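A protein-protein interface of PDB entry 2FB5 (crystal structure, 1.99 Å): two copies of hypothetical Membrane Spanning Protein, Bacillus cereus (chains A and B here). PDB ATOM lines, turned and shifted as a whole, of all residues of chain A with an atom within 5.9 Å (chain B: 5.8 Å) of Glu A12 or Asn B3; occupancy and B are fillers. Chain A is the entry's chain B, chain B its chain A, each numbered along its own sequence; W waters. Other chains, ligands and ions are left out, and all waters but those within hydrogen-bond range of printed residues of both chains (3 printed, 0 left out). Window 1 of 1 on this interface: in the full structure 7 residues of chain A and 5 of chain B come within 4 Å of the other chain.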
ATOM      1  N   GLU A   7     -28.586   7.093 -19.980  1.00  0.00           N
ATOM      2  CA  GLU A   7     -27.562   8.145 -20.055  1.00  0.00           C
ATOM      3  C   GLU A   7     -26.424   7.769 -21.014  1.00  0.00           C
ATOM      4  O   GLU A   7     -25.839   8.636 -21.679  1.00  0.00           O
ATOM      5  CB  GLU A   7     -27.009   8.467 -18.652  1.00  0.00           C
ATOM      6  CG  GLU A   7     -28.037   9.132 -17.700  1.00  0.00           C
ATOM      7  CD  GLU A   7     -28.631  10.425 -18.253  1.00  0.00           C
ATOM      8  OE1 GLU A   7     -27.859  11.278 -18.746  1.00  0.00           O
ATOM      9  OE2 GLU A   7     -29.875  10.596 -18.202  1.00  0.00           O
ATOM     10  N   TRP A   8     -26.102   6.479 -21.068  1.00  0.00           N
ATOM     11  CA  TRP A   8     -25.073   5.991 -21.976  1.00  0.00           C
ATOM     12  C   TRP A   8     -25.486   6.212 -23.432  1.00  0.00           C
ATOM     13  O   TRP A   8     -24.680   6.657 -24.252  1.00  0.00           O
ATOM     14  CB  TRP A   8     -24.795   4.522 -21.736  1.00  0.00           C
ATOM     15  CG  TRP A   8     -23.605   4.037 -22.476  1.00  0.00           C
ATOM     16  CD1 TRP A   8     -22.484   4.760 -22.794  1.00  0.00           C
ATOM     17  CD2 TRP A   8     -23.389   2.719 -22.975  1.00  0.00           C
ATOM     18  NE1 TRP A   8     -21.596   3.971 -23.478  1.00  0.00           N
ATOM     19  CE2 TRP A   8     -22.122   2.711 -23.596  1.00  0.00           C
ATOM     20  CE3 TRP A   8     -24.145   1.540 -22.959  1.00  0.00           C
ATOM     21  CZ2 TRP A   8     -21.581   1.562 -24.187  1.00  0.00           C
ATOM     22  CZ3 TRP A   8     -23.611   0.398 -23.562  1.00  0.00           C
ATOM     23  CH2 TRP A   8     -22.341   0.423 -24.167  1.00  0.00           C
ATOM     24  N   GLY A   9     -26.741   5.895 -23.736  1.00  0.00           N
ATOM     25  CA  GLY A   9     -27.332   6.211 -25.031  1.00  0.00           C
ATOM     26  C   GLY A   9     -27.239   7.693 -25.349  1.00  0.00           C
ATOM     27  O   GLY A   9     -26.939   8.063 -26.480  1.00  0.00           O
ATOM     28  N   LEU A  10     -27.492   8.553 -24.362  1.00  0.00           N
ATOM     29  CA  LEU A  10     -27.413   9.999 -24.611  1.00  0.00           C
ATOM     30  C   LEU A  10     -25.980  10.441 -24.889  1.00  0.00           C
ATOM     31  O   LEU A  10     -25.743  11.233 -25.796  1.00  0.00           O
ATOM     32  CB  LEU A  10     -28.003  10.803 -23.451  1.00  0.00           C
ATOM     33  CG  LEU A  10     -29.489  10.575 -23.126  1.00  0.00           C
ATOM     34  CD1 LEU A  10     -29.890  11.421 -21.911  1.00  0.00           C
ATOM     35  CD2 LEU A  10     -30.456  10.830 -24.326  1.00  0.00           C
ATOM     36  N   SER A  11     -25.033   9.922 -24.107  1.00  0.00           N
ATOM     37  CA  SER A  11     -23.628  10.206 -24.318  1.00  0.00           C
ATOM     38  C   SER A  11     -23.236   9.809 -25.731  1.00  0.00           C
ATOM     39  O   SER A  11     -22.601  10.582 -26.449  1.00  0.00           O
ATOM     40  CB  SER A  11     -22.777   9.431 -23.316  1.00  0.00           C
ATOM     41  OG  SER A  11     -23.074   9.838 -21.992  1.00  0.00           O
ATOM     42  N   GLU A  12     -23.647   8.606 -26.129  1.00  0.00           N
ATOM     43  CA  GLU A  12     -23.268   8.061 -27.420  1.00  0.00           C
ATOM     44  C   GLU A  12     -23.848   8.877 -28.566  1.00  0.00           C
ATOM     45  O   GLU A  12     -23.195   9.028 -29.595  1.00  0.00           O
ATOM     46  CB  GLU A  12     -23.681   6.587 -27.536  1.00  0.00           C
ATOM     47  CG  GLU A  12     -22.763   5.649 -26.774  1.00  0.00           C
ATOM     48  CD  GLU A  12     -21.385   5.554 -27.406  1.00  0.00           C
ATOM     49  OE1 GLU A  12     -21.288   5.184 -28.606  1.00  0.00           O
ATOM     50  OE2 GLU A  12     -20.409   5.868 -26.700  1.00  0.00           O
ATOM     51  N   GLU A  13     -25.048   9.420 -28.384  1.00  0.00           N
ATOM     52  CA  GLU A  13     -25.627  10.279 -29.414  1.00  0.00           C
ATOM     53  C   GLU A  13     -24.915  11.628 -29.530  1.00  0.00           C
ATOM     54  O   GLU A  13     -24.803  12.178 -30.629  1.00  0.00           O
ATOM     55  CB  GLU A  13     -27.127  10.487 -29.197  1.00  0.00           C
ATOM     56  CG  GLU A  13     -27.981   9.263 -29.541  1.00  0.00           C
ATOM     57  CD  GLU A  13     -27.908   8.837 -31.020  1.00  0.00           C
ATOM     58  OE1 GLU A  13     -27.981   7.605 -31.284  1.00  0.00           O
ATOM     59  OE2 GLU A  13     -27.785   9.727 -31.913  1.00  0.00           O
ATOM     60  N   LEU A  14     -24.444  12.158 -28.403  1.00  0.00           N
ATOM     61  CA  LEU A  14     -23.662  13.399 -28.405  1.00  0.00           C
ATOM     62  C   LEU A  14     -22.331  13.216 -29.128  1.00  0.00           C
ATOM     63  O   LEU A  14     -21.879  14.120 -29.854  1.00  0.00           O
ATOM     64  CB  LEU A  14     -23.430  13.903 -26.979  1.00  0.00           C
ATOM     65  CG  LEU A  14     -24.670  14.504 -26.291  1.00  0.00           C
ATOM     66  CD1 LEU A  14     -24.348  14.821 -24.823  1.00  0.00           C
ATOM     67  CD2 LEU A  14     -25.191  15.735 -27.038  1.00  0.00           C
ATOM     68  N   LYS A  15     -21.727  12.041 -28.929  1.00  0.00           N
ATOM     69  CA  LYS A  15     -20.521  11.634 -29.649  1.00  0.00           C
ATOM     70  C   LYS A  15     -20.773  11.571 -31.160  1.00  0.00           C
ATOM     71  O   LYS A  15     -19.967  12.067 -31.951  1.00  0.00           O
ATOM     72  CB  LYS A  15     -20.011  10.291 -29.120  1.00  0.00           C
ATOM     73  CG  LYS A  15     -18.661   9.847 -29.715  1.00  0.00           C
ATOM     74  CD  LYS A  15     -17.908   8.920 -28.760  1.00  0.00           C
ATOM     75  CE  LYS A  15     -18.442   7.496 -28.814  1.00  0.00           C
ATOM     76  NZ  LYS A  15     -17.644   6.668 -27.885  1.00  0.00           N
ATOM     77  N   ILE A  16     -21.898  10.973 -31.550  1.00  0.00           N
ATOM     78  CA  ILE A  16     -22.317  10.928 -32.952  1.00  0.00           C
ATOM     79  C   ILE A  16     -22.454  12.328 -33.552  1.00  0.00           C
ATOM     80  O   ILE A  16     -21.959  12.583 -34.646  1.00  0.00           O
ATOM     81  CB  ILE A  16     -23.640  10.144 -33.112  1.00  0.00           C
ATOM     82  CG1 ILE A  16     -23.384   8.646 -32.915  1.00  0.00           C
ATOM     83  CG2 ILE A  16     -24.311  10.451 -34.476  1.00  0.00           C
ATOM     84  CD1 ILE A  16     -24.678   7.781 -32.848  1.00  0.00           C
ATOM     85  N   GLN A  17     -23.112  13.226 -32.829  1.00  0.00           N
ATOM     86  CA  GLN A  17     -23.290  14.606 -33.286  1.00  0.00           C
ATOM     87  C   GLN A  17     -21.968  15.350 -33.435  1.00  0.00           C
ATOM     88  O   GLN A  17     -21.802  16.144 -34.357  1.00  0.00           O
ATOM     89  CB  GLN A  17     -24.199  15.370 -32.331  1.00  0.00           C
ATOM     90  CG  GLN A  17     -25.668  14.939 -32.348  1.00  0.00           C
ATOM     91  CD  GLN A  17     -26.432  15.530 -31.159  1.00  0.00           C
ATOM     92  OE1 GLN A  17     -26.387  16.737 -30.918  1.00  0.00           O
ATOM     93  NE2 GLN A  17     -27.092  14.674 -30.386  1.00  0.00           N
ATOM     94  N   TYR A  64     -20.554  16.700 -25.048  1.00  0.00           N
ATOM     95  CA  TYR A  64     -20.274  15.270 -24.958  1.00  0.00           C
ATOM     96  C   TYR A  64     -19.486  14.910 -23.702  1.00  0.00           C
ATOM     97  O   TYR A  64     -19.891  14.025 -22.945  1.00  0.00           O
ATOM     98  CB  TYR A  64     -19.518  14.727 -26.194  1.00  0.00           C
ATOM     99  CG  TYR A  64     -19.016  13.325 -25.940  1.00  0.00           C
ATOM    100  CD1 TYR A  64     -19.913  12.265 -25.797  1.00  0.00           C
ATOM    101  CD2 TYR A  64     -17.656  13.061 -25.782  1.00  0.00           C
ATOM    102  CE1 TYR A  64     -19.468  10.986 -25.530  1.00  0.00           C
ATOM    103  CE2 TYR A  64     -17.205  11.785 -25.511  1.00  0.00           C
ATOM    104  CZ  TYR A  64     -18.121  10.752 -25.392  1.00  0.00           C
ATOM    105  OH  TYR A  64     -17.692   9.483 -25.128  1.00  0.00           O
ATOM    106  N   SER B   2     -23.605   2.846 -34.532  1.00  0.00           N
ATOM    107  CA  SER B   2     -22.431   3.355 -33.780  1.00  0.00           C
ATOM    108  C   SER B   2     -22.734   3.936 -32.394  1.00  0.00           C
ATOM    109  O   SER B   2     -21.807   4.240 -31.637  1.00  0.00           O
ATOM    110  CB  SER B   2     -21.722   4.409 -34.579  1.00  0.00           C
ATOM    111  OG  SER B   2     -20.476   4.663 -33.984  1.00  0.00           O
ATOM    112  N   ASN B   3     -24.010   4.096 -32.072  1.00  0.00           N
ATOM    113  CA  ASN B   3     -24.434   4.251 -30.685  1.00  0.00           C
ATOM    114  C   ASN B   3     -24.127   2.927 -29.951  1.00  0.00           C
ATOM    115  O   ASN B   3     -24.797   1.929 -30.163  1.00  0.00           O
ATOM    116  CB  ASN B   3     -25.933   4.590 -30.644  1.00  0.00           C
ATOM    117  CG  ASN B   3     -26.429   4.953 -29.246  1.00  0.00           C
ATOM    118  OD1 ASN B   3     -27.153   5.941 -29.065  1.00  0.00           O
ATOM    119  ND2 ASN B   3     -26.061   4.160 -28.262  1.00  0.00           N
ATOM    120  N   ALA B   4     -23.092   2.920 -29.111  1.00  0.00           N
ATOM    121  CA  ALA B   4     -22.685   1.697 -28.411  1.00  0.00           C
ATOM    122  C   ALA B   4     -23.788   1.030 -27.560  1.00  0.00           C
ATOM    123  O   ALA B   4     -23.812  -0.199 -27.436  1.00  0.00           O
ATOM    124  CB  ALA B   4     -21.419   1.943 -27.560  1.00  0.00           C
ATOM    125  N   MET B   5     -24.677   1.827 -26.965  1.00  0.00           N
ATOM    126  CA  MET B   5     -25.792   1.288 -26.182  1.00  0.00           C
ATOM    127  C   MET B   5     -26.693   0.475 -27.110  1.00  0.00           C
ATOM    128  O   MET B   5     -26.983  -0.697 -26.830  1.00  0.00           O
ATOM    129  CB  MET B   5     -26.587   2.408 -25.486  1.00  0.00           C
ATOM    130  CG  MET B   5     -27.710   1.928 -24.525  1.00  0.00           C
ATOM    131  SD  MET B   5     -29.157   3.016 -24.436  1.00  0.00           S
ATOM    132  CE  MET B   5     -29.865   2.759 -26.059  1.00  0.00           C
ATOM    133  N   HIS B   6     -27.108   1.091 -28.219  1.00  0.00           N
ATOM    134  CA  HIS B   6     -27.931   0.427 -29.231  1.00  0.00           C
ATOM    135  C   HIS B   6     -27.251  -0.831 -29.781  1.00  0.00           C
ATOM    136  O   HIS B   6     -27.872  -1.892 -29.839  1.00  0.00           O
ATOM    137  CB  HIS B   6     -28.299   1.413 -30.356  1.00  0.00           C
ATOM    138  CG  HIS B   6     -29.150   0.826 -31.442  1.00  0.00           C
ATOM    139  ND1 HIS B   6     -30.529   0.809 -31.386  1.00  0.00           N
ATOM    140  CD2 HIS B   6     -28.817   0.271 -32.634  1.00  0.00           C
ATOM    141  CE1 HIS B   6     -31.009   0.249 -32.484  1.00  0.00           C
ATOM    142  NE2 HIS B   6     -29.992  -0.086 -33.258  1.00  0.00           N
ATOM    143  N   GLU B   7     -25.975  -0.719 -30.147  1.00  0.00           N
ATOM    144  CA  GLU B   7     -25.216  -1.851 -30.701  1.00  0.00           C
ATOM    145  C   GLU B   7     -25.095  -3.005 -29.703  1.00  0.00           C
ATOM    146  O   GLU B   7     -25.078  -4.175 -30.095  1.00  0.00           O
ATOM    147  CB  GLU B   7     -23.813  -1.403 -31.165  1.00  0.00           C
ATOM    148  CG  GLU B   7     -23.813  -0.445 -32.378  1.00  0.00           C
ATOM    149  CD  GLU B   7     -24.556  -1.012 -33.579  1.00  0.00           C
ATOM    150  OE1 GLU B   7     -24.318  -2.191 -33.937  1.00  0.00           O
ATOM    151  OE2 GLU B   7     -25.386  -0.287 -34.174  1.00  0.00           O
ATOM    152  N   TRP B   8     -24.981  -2.669 -28.420  1.00  0.00           N
ATOM    153  CA  TRP B   8     -24.913  -3.683 -27.375  1.00  0.00           C
ATOM    154  C   TRP B   8     -26.214  -4.494 -27.312  1.00  0.00           C
ATOM    155  O   TRP B   8     -26.192  -5.732 -27.245  1.00  0.00           O
ATOM    156  CB  TRP B   8     -24.637  -3.048 -26.031  1.00  0.00           C
ATOM    157  CG  TRP B   8     -24.335  -4.053 -24.977  1.00  0.00           C
ATOM    158  CD1 TRP B   8     -23.743  -5.270 -25.151  1.00  0.00           C
ATOM    159  CD2 TRP B   8     -24.601  -3.929 -23.580  1.00  0.00           C
ATOM    160  NE1 TRP B   8     -23.637  -5.918 -23.949  1.00  0.00           N
ATOM    161  CE2 TRP B   8     -24.152  -5.116 -22.965  1.00  0.00           C
ATOM    162  CE3 TRP B   8     -25.177  -2.929 -22.786  1.00  0.00           C
ATOM    163  CZ2 TRP B   8     -24.239  -5.329 -21.582  1.00  0.00           C
ATOM    164  CZ3 TRP B   8     -25.277  -3.146 -21.411  1.00  0.00           C
ATOM    165  CH2 TRP B   8     -24.816  -4.342 -20.827  1.00  0.00           C
HETATM  166  O   HOH W   1     -29.949   6.510 -27.098  1.00  0.00           O
HETATM  167  O   HOH W   2     -19.433   3.735 -30.041  1.00  0.00           O
HETATM  168  O   HOH W   3     -21.370   7.228 -30.543  1.00  0.00           O
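The side-chain carboxylate of Glu A12 lies within hydrogen-bond range of the backbone NH of Ala B4.
O of Gly A9 lies close to OD1 of Asn B3.
OD1 of Asn B3 sits close to OE1 of Glu A13 (2.9 Å).
OE1 of Glu A12 sits close to O of Ser B2 (3.2 Å).
The side-chain carboxylate (OE2) of Glu A12 is in salt-bridge range of the side-chain amino group (NZ) of Lys A15 (3.1 Å).
O of Glu A13 sits close to NE2 of Gln A17, 3.4 Å away.
ND2 of Asn B3 sits close to N of His B6, 3.2 Å away.
The backbone NH of Met B5 sits close to the side-chain amide nitrogen of Asn B3 (3.0 Å).
Among the printed residues, pairs that only touch across the chains: Trp A8 with Ala B4, Trp A8 with Met B5, Trp A8 with Trp B8, Gly A9 with Met B5, Glu A12 with Asn B3 and Ile A16 with Asn B3.
Leu A10 touches none of the printed residues of chain B.
Glu A12 touches just these residues of chain B: Ser B2, Asn B3 and Ala B4.
Of the printed residues of chain A, Ser B2 touches Glu A12 (3.2 Å).
Asn B3 touches just these residues of chain A: Gly A9 (3.4 Å), Glu A12 (3.5 Å), Glu A13 (2.9 Å) and Ile A16 (3.8 Å).
Printed residues of chain A within 4 Å of Met B5: Trp A8 (3.5 Å) and Gly A9 (3.7 Å).
Of the 7 printed residues of chain B, 5 touch a printed residue of chain A.
Along chain B the printed residues that touch a printed residue of chain A span positions 2 to 8.
Of the 12 printed residues of chain A, 5 touch a printed residue of chain B.
Printed residues of chain A that touch a printed residue of chain B: Trp A8, Gly A9, Glu A12, Glu A13 and Ile A16.
Trp A8 touches its own counterpart, Trp B8.
2 positions are printed for both chains.
Of the 10 pairs that touch across the chains among the printed residues, 1 has its exchanged pair printed and touching as well.
Water W3 bridges O of Glu A12 (2.7 Å) and O of Ser B2 (3.2 Å).
Water W2 bridges the side-chain carboxylate of Glu A12 and the backbone carbonyl oxygen of Ser B2.
Water W1 lies within hydrogen-bond range of the backbone carbonyl oxygen (O) of Gly A9 (3.4 Å) and the side-chain amide oxygen (OD1) of Asn B3 (3.5 Å).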
